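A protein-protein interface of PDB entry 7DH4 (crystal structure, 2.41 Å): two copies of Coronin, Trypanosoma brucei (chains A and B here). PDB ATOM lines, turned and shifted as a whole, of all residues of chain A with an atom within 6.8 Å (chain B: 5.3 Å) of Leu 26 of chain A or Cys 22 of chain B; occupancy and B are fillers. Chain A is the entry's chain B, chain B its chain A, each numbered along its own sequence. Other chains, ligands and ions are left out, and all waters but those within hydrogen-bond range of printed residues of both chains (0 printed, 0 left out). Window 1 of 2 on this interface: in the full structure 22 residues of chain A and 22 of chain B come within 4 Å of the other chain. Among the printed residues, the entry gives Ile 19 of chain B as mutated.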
ATOM      1  N   ARG A  21      -1.376   3.483  26.730  1.00  0.00           N
ATOM      2  CA  ARG A  21      -2.129   3.726  27.955  1.00  0.00           C
ATOM      3  C   ARG A  21      -1.910   5.151  28.444  1.00  0.00           C
ATOM      4  O   ARG A  21      -2.856   5.822  28.870  1.00  0.00           O
ATOM      5  CB  ARG A  21      -1.726   2.716  29.033  1.00  0.00           C
ATOM      6  N   CYS A  22      -0.666   5.631  28.377  1.00  0.00           N
ATOM      7  CA  CYS A  22      -0.381   7.013  28.741  1.00  0.00           C
ATOM      8  C   CYS A  22      -1.040   7.991  27.779  1.00  0.00           C
ATOM      9  O   CYS A  22      -1.449   9.083  28.188  1.00  0.00           O
ATOM     10  CB  CYS A  22       1.130   7.240  28.776  1.00  0.00           C
ATOM     11  SG  CYS A  22       1.628   8.950  29.090  1.00  0.00           S
ATOM     12  N   ARG A  23      -1.159   7.621  26.501  1.00  0.00           N
ATOM     13  CA  ARG A  23      -1.727   8.541  25.523  1.00  0.00           C
ATOM     14  C   ARG A  23      -3.243   8.632  25.649  1.00  0.00           C
ATOM     15  O   ARG A  23      -3.805   9.730  25.589  1.00  0.00           O
ATOM     16  CB  ARG A  23      -1.329   8.125  24.105  1.00  0.00           C
ATOM     17  CG  ARG A  23      -2.024   8.949  23.042  1.00  0.00           C
ATOM     18  CD  ARG A  23      -1.175   9.162  21.797  1.00  0.00           C
ATOM     19  NE  ARG A  23      -0.134   8.156  21.621  1.00  0.00           N
ATOM     20  CZ  ARG A  23       1.142   8.438  21.386  1.00  0.00           C
ATOM     21  NH1 ARG A  23       1.544   9.700  21.311  1.00  0.00           N
ATOM     22  NH2 ARG A  23       2.015   7.459  21.226  1.00  0.00           N
ATOM     23  N   GLU A  24      -3.923   7.496  25.820  1.00  0.00           N
ATOM     24  CA  GLU A  24      -5.358   7.535  26.089  1.00  0.00           C
ATOM     25  C   GLU A  24      -5.654   8.307  27.366  1.00  0.00           C
ATOM     26  O   GLU A  24      -6.681   8.989  27.457  1.00  0.00           O
ATOM     27  CB  GLU A  24      -5.917   6.113  26.179  1.00  0.00           C
ATOM     28  N   ASP A  25      -4.768   8.213  28.357  1.00  0.00           N
ATOM     29  CA  ASP A  25      -4.886   9.046  29.548  1.00  0.00           C
ATOM     30  C   ASP A  25      -4.791  10.527  29.191  1.00  0.00           C
ATOM     31  O   ASP A  25      -5.609  11.339  29.636  1.00  0.00           O
ATOM     32  CB  ASP A  25      -3.801   8.656  30.553  1.00  0.00           C
ATOM     33  CG  ASP A  25      -3.862   9.469  31.827  1.00  0.00           C
ATOM     34  OD1 ASP A  25      -4.585   9.063  32.762  1.00  0.00           O
ATOM     35  OD2 ASP A  25      -3.180  10.514  31.894  1.00  0.00           O
ATOM     36  N   LEU A  26      -3.799  10.885  28.373  1.00  0.00           N
ATOM     37  CA  LEU A  26      -3.612  12.285  27.996  1.00  0.00           C
ATOM     38  C   LEU A  26      -4.807  12.815  27.218  1.00  0.00           C
ATOM     39  O   LEU A  26      -5.245  13.951  27.438  1.00  0.00           O
ATOM     40  CB  LEU A  26      -2.330  12.431  27.175  1.00  0.00           C
ATOM     41  CG  LEU A  26      -1.990  13.807  26.594  1.00  0.00           C
ATOM     42  CD1 LEU A  26      -1.763  14.826  27.697  1.00  0.00           C
ATOM     43  CD2 LEU A  26      -0.773  13.721  25.682  1.00  0.00           C
ATOM     44  N   GLN A  27      -5.356  12.007  26.309  1.00  0.00           N
ATOM     45  CA  GLN A  27      -6.420  12.491  25.436  1.00  0.00           C
ATOM     46  C   GLN A  27      -7.727  12.699  26.189  1.00  0.00           C
ATOM     47  O   GLN A  27      -8.525  13.566  25.813  1.00  0.00           O
ATOM     48  CB  GLN A  27      -6.608  11.523  24.269  1.00  0.00           C
ATOM     49  CG  GLN A  27      -5.414  11.494  23.328  1.00  0.00           C
ATOM     50  CD  GLN A  27      -5.433  10.314  22.380  1.00  0.00           C
ATOM     51  OE1 GLN A  27      -6.283   9.430  22.486  1.00  0.00           O
ATOM     52  NE2 GLN A  27      -4.496  10.297  21.439  1.00  0.00           N
ATOM     53  N   LYS A  28      -7.968  11.923  27.249  1.00  0.00           N
ATOM     54  CA  LYS A  28      -9.124  12.189  28.099  1.00  0.00           C
ATOM     55  C   LYS A  28      -8.971  13.520  28.821  1.00  0.00           C
ATOM     56  O   LYS A  28      -9.952  14.248  29.016  1.00  0.00           O
ATOM     57  CB  LYS A  28      -9.313  11.051  29.102  1.00  0.00           C
ATOM     58  N   LYS A  29      -7.741  13.858  29.220  1.00  0.00           N
ATOM     59  CA  LYS A  29      -7.505  15.126  29.899  1.00  0.00           C
ATOM     60  C   LYS A  29      -7.621  16.301  28.937  1.00  0.00           C
ATOM     61  O   LYS A  29      -8.194  17.340  29.285  1.00  0.00           O
ATOM     62  CB  LYS A  29      -6.130  15.115  30.563  1.00  0.00           C
ATOM     63  CG  LYS A  29      -6.113  14.491  31.945  1.00  0.00           C
ATOM     64  CD  LYS A  29      -4.709  14.504  32.524  1.00  0.00           C
ATOM     65  CE  LYS A  29      -4.364  13.167  33.150  1.00  0.00           C
ATOM     66  NZ  LYS A  29      -2.941  12.801  32.909  1.00  0.00           N
ATOM     67  N   GLU A  30      -7.074  16.158  27.726  1.00  0.00           N
ATOM     68  CA  GLU A  30      -7.242  17.195  26.714  1.00  0.00           C
ATOM     69  C   GLU A  30      -8.715  17.410  26.395  1.00  0.00           C
ATOM     70  O   GLU A  30      -9.155  18.547  26.184  1.00  0.00           O
ATOM     71  CB  GLU A  30      -6.472  16.825  25.445  1.00  0.00           C
ATOM     72  CG  GLU A  30      -4.964  16.708  25.624  1.00  0.00           C
ATOM     73  CD  GLU A  30      -4.273  16.179  24.378  1.00  0.00           C
ATOM     74  OE1 GLU A  30      -4.841  15.285  23.716  1.00  0.00           O
ATOM     75  OE2 GLU A  30      -3.162  16.656  24.058  1.00  0.00           O
ATOM     76  N   SER A  31      -9.494  16.325  26.359  1.00  0.00           N
ATOM     77  CA  SER A  31     -10.920  16.446  26.082  1.00  0.00           C
ATOM     78  C   SER A  31     -11.658  17.129  27.225  1.00  0.00           C
ATOM     79  O   SER A  31     -12.625  17.861  26.986  1.00  0.00           O
ATOM     80  CB  SER A  31     -11.518  15.067  25.809  1.00  0.00           C
ATOM     81  OG  SER A  31     -12.933  15.116  25.785  1.00  0.00           O
ATOM     82  N   LEU A  32     -11.223  16.903  28.467  1.00  0.00           N
ATOM     83  CA  LEU A  32     -11.835  17.582  29.602  1.00  0.00           C
ATOM     84  C   LEU A  32     -11.421  19.046  29.674  1.00  0.00           C
ATOM     85  O   LEU A  32     -12.219  19.892  30.092  1.00  0.00           O
ATOM     86  CB  LEU A  32     -11.470  16.864  30.902  1.00  0.00           C
ATOM     87  CG  LEU A  32     -12.472  15.807  31.371  1.00  0.00           C
ATOM     88  CD1 LEU A  32     -11.933  15.041  32.567  1.00  0.00           C
ATOM     89  CD2 LEU A  32     -13.814  16.447  31.697  1.00  0.00           C
ATOM     90  N   GLU B  18      -1.311  20.357  34.158  1.00  0.00           N
ATOM     91  CA  GLU B  18      -1.338  18.906  34.302  1.00  0.00           C
ATOM     92  C   GLU B  18      -1.135  18.216  32.958  1.00  0.00           C
ATOM     93  O   GLU B  18      -0.395  17.229  32.866  1.00  0.00           O
ATOM     94  CB  GLU B  18      -2.661  18.480  34.938  1.00  0.00           C
ATOM     95  CG  GLU B  18      -2.872  16.984  35.052  1.00  0.00           C
ATOM     96  CD  GLU B  18      -4.237  16.641  35.614  1.00  0.00           C
ATOM     97  OE1 GLU B  18      -4.608  15.449  35.584  1.00  0.00           O
ATOM     98  OE2 GLU B  18      -4.938  17.561  36.085  1.00  0.00           O
ATOM     99  N   ILE B  19      -1.775  18.731  31.904  1.00  0.00           N
ATOM    100  CA  ILE B  19      -1.607  18.154  30.572  1.00  0.00           C
ATOM    101  C   ILE B  19      -0.172  18.329  30.091  1.00  0.00           C
ATOM    102  O   ILE B  19       0.405  17.427  29.469  1.00  0.00           O
ATOM    103  CB  ILE B  19      -2.618  18.781  29.594  1.00  0.00           C
ATOM    104  CG1 ILE B  19      -4.002  18.164  29.801  1.00  0.00           C
ATOM    105  CG2 ILE B  19      -2.158  18.619  28.150  1.00  0.00           C
ATOM    106  CD1 ILE B  19      -5.131  19.100  29.459  1.00  0.00           C
ATOM    107  N   GLN B  20       0.432  19.484  30.382  1.00  0.00           N
ATOM    108  CA  GLN B  20       1.792  19.739  29.919  1.00  0.00           C
ATOM    109  C   GLN B  20       2.794  18.810  30.595  1.00  0.00           C
ATOM    110  O   GLN B  20       3.786  18.405  29.977  1.00  0.00           O
ATOM    111  CB  GLN B  20       2.166  21.202  30.157  1.00  0.00           C
ATOM    112  CG  GLN B  20       1.778  22.118  29.009  1.00  0.00           C
ATOM    113  CD  GLN B  20       1.930  23.584  29.354  1.00  0.00           C
ATOM    114  OE1 GLN B  20       1.326  24.077  30.306  1.00  0.00           O
ATOM    115  NE2 GLN B  20       2.738  24.292  28.575  1.00  0.00           N
ATOM    116  N   ARG B  21       2.557  18.463  31.861  1.00  0.00           N
ATOM    117  CA  ARG B  21       3.406  17.470  32.511  1.00  0.00           C
ATOM    118  C   ARG B  21       3.213  16.093  31.891  1.00  0.00           C
ATOM    119  O   ARG B  21       4.173  15.327  31.751  1.00  0.00           O
ATOM    120  CB  ARG B  21       3.124  17.423  34.013  1.00  0.00           C
ATOM    121  CG  ARG B  21       4.108  18.218  34.852  1.00  0.00           C
ATOM    122  CD  ARG B  21       3.382  19.103  35.851  1.00  0.00           C
ATOM    123  NE  ARG B  21       2.496  18.333  36.721  1.00  0.00           N
ATOM    124  CZ  ARG B  21       1.407  18.821  37.306  1.00  0.00           C
ATOM    125  NH1 ARG B  21       0.665  18.043  38.082  1.00  0.00           N
ATOM    126  NH2 ARG B  21       1.056  20.086  37.113  1.00  0.00           N
ATOM    127  N   CYS B  22       1.976  15.760  31.513  1.00  0.00           N
ATOM    128  CA  CYS B  22       1.718  14.466  30.890  1.00  0.00           C
ATOM    129  C   CYS B  22       2.367  14.375  29.516  1.00  0.00           C
ATOM    130  O   CYS B  22       2.883  13.317  29.135  1.00  0.00           O
ATOM    131  CB  CYS B  22       0.213  14.221  30.791  1.00  0.00           C
ATOM    132  SG  CYS B  22      -0.577  13.823  32.366  1.00  0.00           S
ATOM    133  N   ARG B  23       2.348  15.474  28.753  1.00  0.00           N
ATOM    134  CA  ARG B  23       3.026  15.485  27.460  1.00  0.00           C
ATOM    135  C   ARG B  23       4.532  15.325  27.618  1.00  0.00           C
ATOM    136  O   ARG B  23       5.183  14.713  26.763  1.00  0.00           O
ATOM    137  CB  ARG B  23       2.717  16.778  26.707  1.00  0.00           C
ATOM    138  CG  ARG B  23       1.324  16.845  26.102  1.00  0.00           C
ATOM    139  CD  ARG B  23       1.097  18.192  25.436  1.00  0.00           C
ATOM    140  NE  ARG B  23      -0.274  18.346  24.959  1.00  0.00           N
ATOM    141  CZ  ARG B  23      -0.888  19.518  24.836  1.00  0.00           C
ATOM    142  NH1 ARG B  23      -0.253  20.637  25.159  1.00  0.00           N
ATOM    143  NH2 ARG B  23      -2.137  19.572  24.399  1.00  0.00           N
ATOM    144  N   GLU B  24       5.099  15.874  28.694  1.00  0.00           N
ATOM    145  CA  GLU B  24       6.519  15.687  28.972  1.00  0.00           C
ATOM    146  C   GLU B  24       6.844  14.213  29.163  1.00  0.00           C
ATOM    147  O   GLU B  24       7.719  13.659  28.487  1.00  0.00           O
ATOM    148  CB  GLU B  24       6.919  16.482  30.215  1.00  0.00           C
ATOM    149  CG  GLU B  24       7.424  17.880  29.934  1.00  0.00           C
ATOM    150  CD  GLU B  24       7.705  18.646  31.208  1.00  0.00           C
ATOM    151  OE1 GLU B  24       7.007  19.648  31.466  1.00  0.00           O
ATOM    152  OE2 GLU B  24       8.619  18.239  31.956  1.00  0.00           O
ATOM    153  N   ASP B  25       6.143  13.559  30.093  1.00  0.00           N
ATOM    154  CA  ASP B  25       6.381  12.142  30.344  1.00  0.00           C
ATOM    155  C   ASP B  25       6.142  11.313  29.089  1.00  0.00           C
ATOM    156  O   ASP B  25       6.954  10.444  28.751  1.00  0.00           O
ATOM    157  CB  ASP B  25       5.501  11.657  31.496  1.00  0.00           C
ATOM    158  CG  ASP B  25       5.780  12.398  32.791  1.00  0.00           C
ATOM    159  OD1 ASP B  25       6.925  12.870  32.966  1.00  0.00           O
ATOM    160  OD2 ASP B  25       4.864  12.504  33.633  1.00  0.00           O
ATOM    161  N   LEU B  26       5.048  11.588  28.370  1.00  0.00           N
ATOM    162  CA  LEU B  26       4.752  10.855  27.140  1.00  0.00           C
ATOM    163  C   LEU B  26       5.922  10.898  26.162  1.00  0.00           C
ATOM    164  O   LEU B  26       6.248   9.887  25.527  1.00  0.00           O
ATOM    165  CB  LEU B  26       3.489  11.421  26.484  1.00  0.00           C
ATOM    166  CG  LEU B  26       2.777  10.621  25.389  1.00  0.00           C
ATOM    167  CD1 LEU B  26       3.371  10.891  24.012  1.00  0.00           C
ATOM    168  CD2 LEU B  26       2.796   9.130  25.691  1.00  0.00           C
ATOM    169  N   GLN B  27       6.570  12.059  26.027  1.00  0.00           N
ATOM    170  CA  GLN B  27       7.675  12.178  25.082  1.00  0.00           C
ATOM    171  C   GLN B  27       8.954  11.541  25.608  1.00  0.00           C
ATOM    172  O   GLN B  27       9.764  11.047  24.815  1.00  0.00           O
ATOM    173  CB  GLN B  27       7.923  13.648  24.739  1.00  0.00           C
ATOM    174  CG  GLN B  27       8.468  13.860  23.336  1.00  0.00           C
ATOM    175  CD  GLN B  27       7.799  15.010  22.610  1.00  0.00           C
ATOM    176  OE1 GLN B  27       7.387  15.994  23.226  1.00  0.00           O
ATOM    177  NE2 GLN B  27       7.683  14.890  21.292  1.00  0.00           N
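SG of Cys 22 of chain B is in hydrogen-bond range of NZ of Lys 29 of chain A. The side-chain carboxylate (OE2) of Glu 30 of chain A lies within salt-bridge range of the guanidinium group (NH2) of Arg 23 of chain B (3.1 Å).
The side-chain sulfur (SG) of Cys 22 of chain B sits at hydrogen-bond distance from the backbone carbonyl oxygen (O) of Glu 18 of chain B (3.4 Å). The side-chain carboxylate (OD2) of Asp 25 of chain A lies within salt-bridge range of the side-chain amino group (NZ) of Lys 29 of chain A (2.5 Å).
Among the printed residues, pairs that only touch across the chains: Cys 22 of chain A with Leu 26 of chain B, Arg 23 of chain A with Leu 26 of chain B, Leu 26 of chain A with Ile 19 of chain B, Leu 26 of chain A with Cys 22 of chain B, Leu 26 of chain A with Arg 23 of chain B, Lys 29 of chain A with Glu 18 of chain B, Lys 29 of chain A with Ile 19 of chain B and Glu 30 of chain A with Ile 19 of chain B.
Cys 22 of chain B touches just these residues of chain A: Leu 26 and Lys 29. Of the printed residues of chain B, Glu 30 of chain A touches Ile 19 and Arg 23. Printed residues of chain A within 4 Å of Ile 19 of chain B: Leu 26 (3.8 Å), Lys 29 (3.5 Å) and Glu 30 (3.9 Å). Of the printed residues of chain A, Leu 26 of chain B touches Cys 22 (3.6 Å) and Arg 23 (3.5 Å). Of the printed residues of chain B, Lys 29 of chain A touches Glu 18 (3.2 Å), Ile 19 (3.5 Å) and Cys 22 (2.6 Å). Asp 25 of chain A touches none of the printed residues of chain B. Glu 24 of chain A touches none of the printed residues of chain B. The nearest residue of chain B that does not touch Leu 26 of chain A is Leu 26 of chain B (4.7 Å). The nearest printed residue of chain B that does not touch Glu 30 of chain A is Gln 20 of chain B (7.7 Å).
Of the 10 printed residues of chain B, 5 touch a printed residue of chain A. Printed residues of chain B that touch a printed residue of chain A: Glu 18, Ile 19, Cys 22, Arg 23 and Leu 26. Hydrophobic or aromatic side chains of chain B that line the printed part of chain A: Ile 19 and Leu 26. Printed residues of chain A that touch a printed residue of chain B: Cys 22, Arg 23, Leu 26, Lys 29 and Glu 30. Among the printed residues, 10 pairs touch across the chains. Among the printed residues, Asp or Glu carboxylates within 4 Å of a Lys or Arg side-chain nitrogen of the other chain: Glu 30 of chain A with Arg 23 of chain B.
Cys 22 of chain A touches Leu 26 of chain B, and with the chains exchanged Leu 26 of chain A touches Cys 22 of chain B. Arg 23 of chain A touches Leu 26 of chain B, and with the chains exchanged Leu 26 of chain A touches Arg 23 of chain B. Of the 10 pairs that touch across the chains among the printed residues, 4 have their exchanged pair printed and touching as well.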
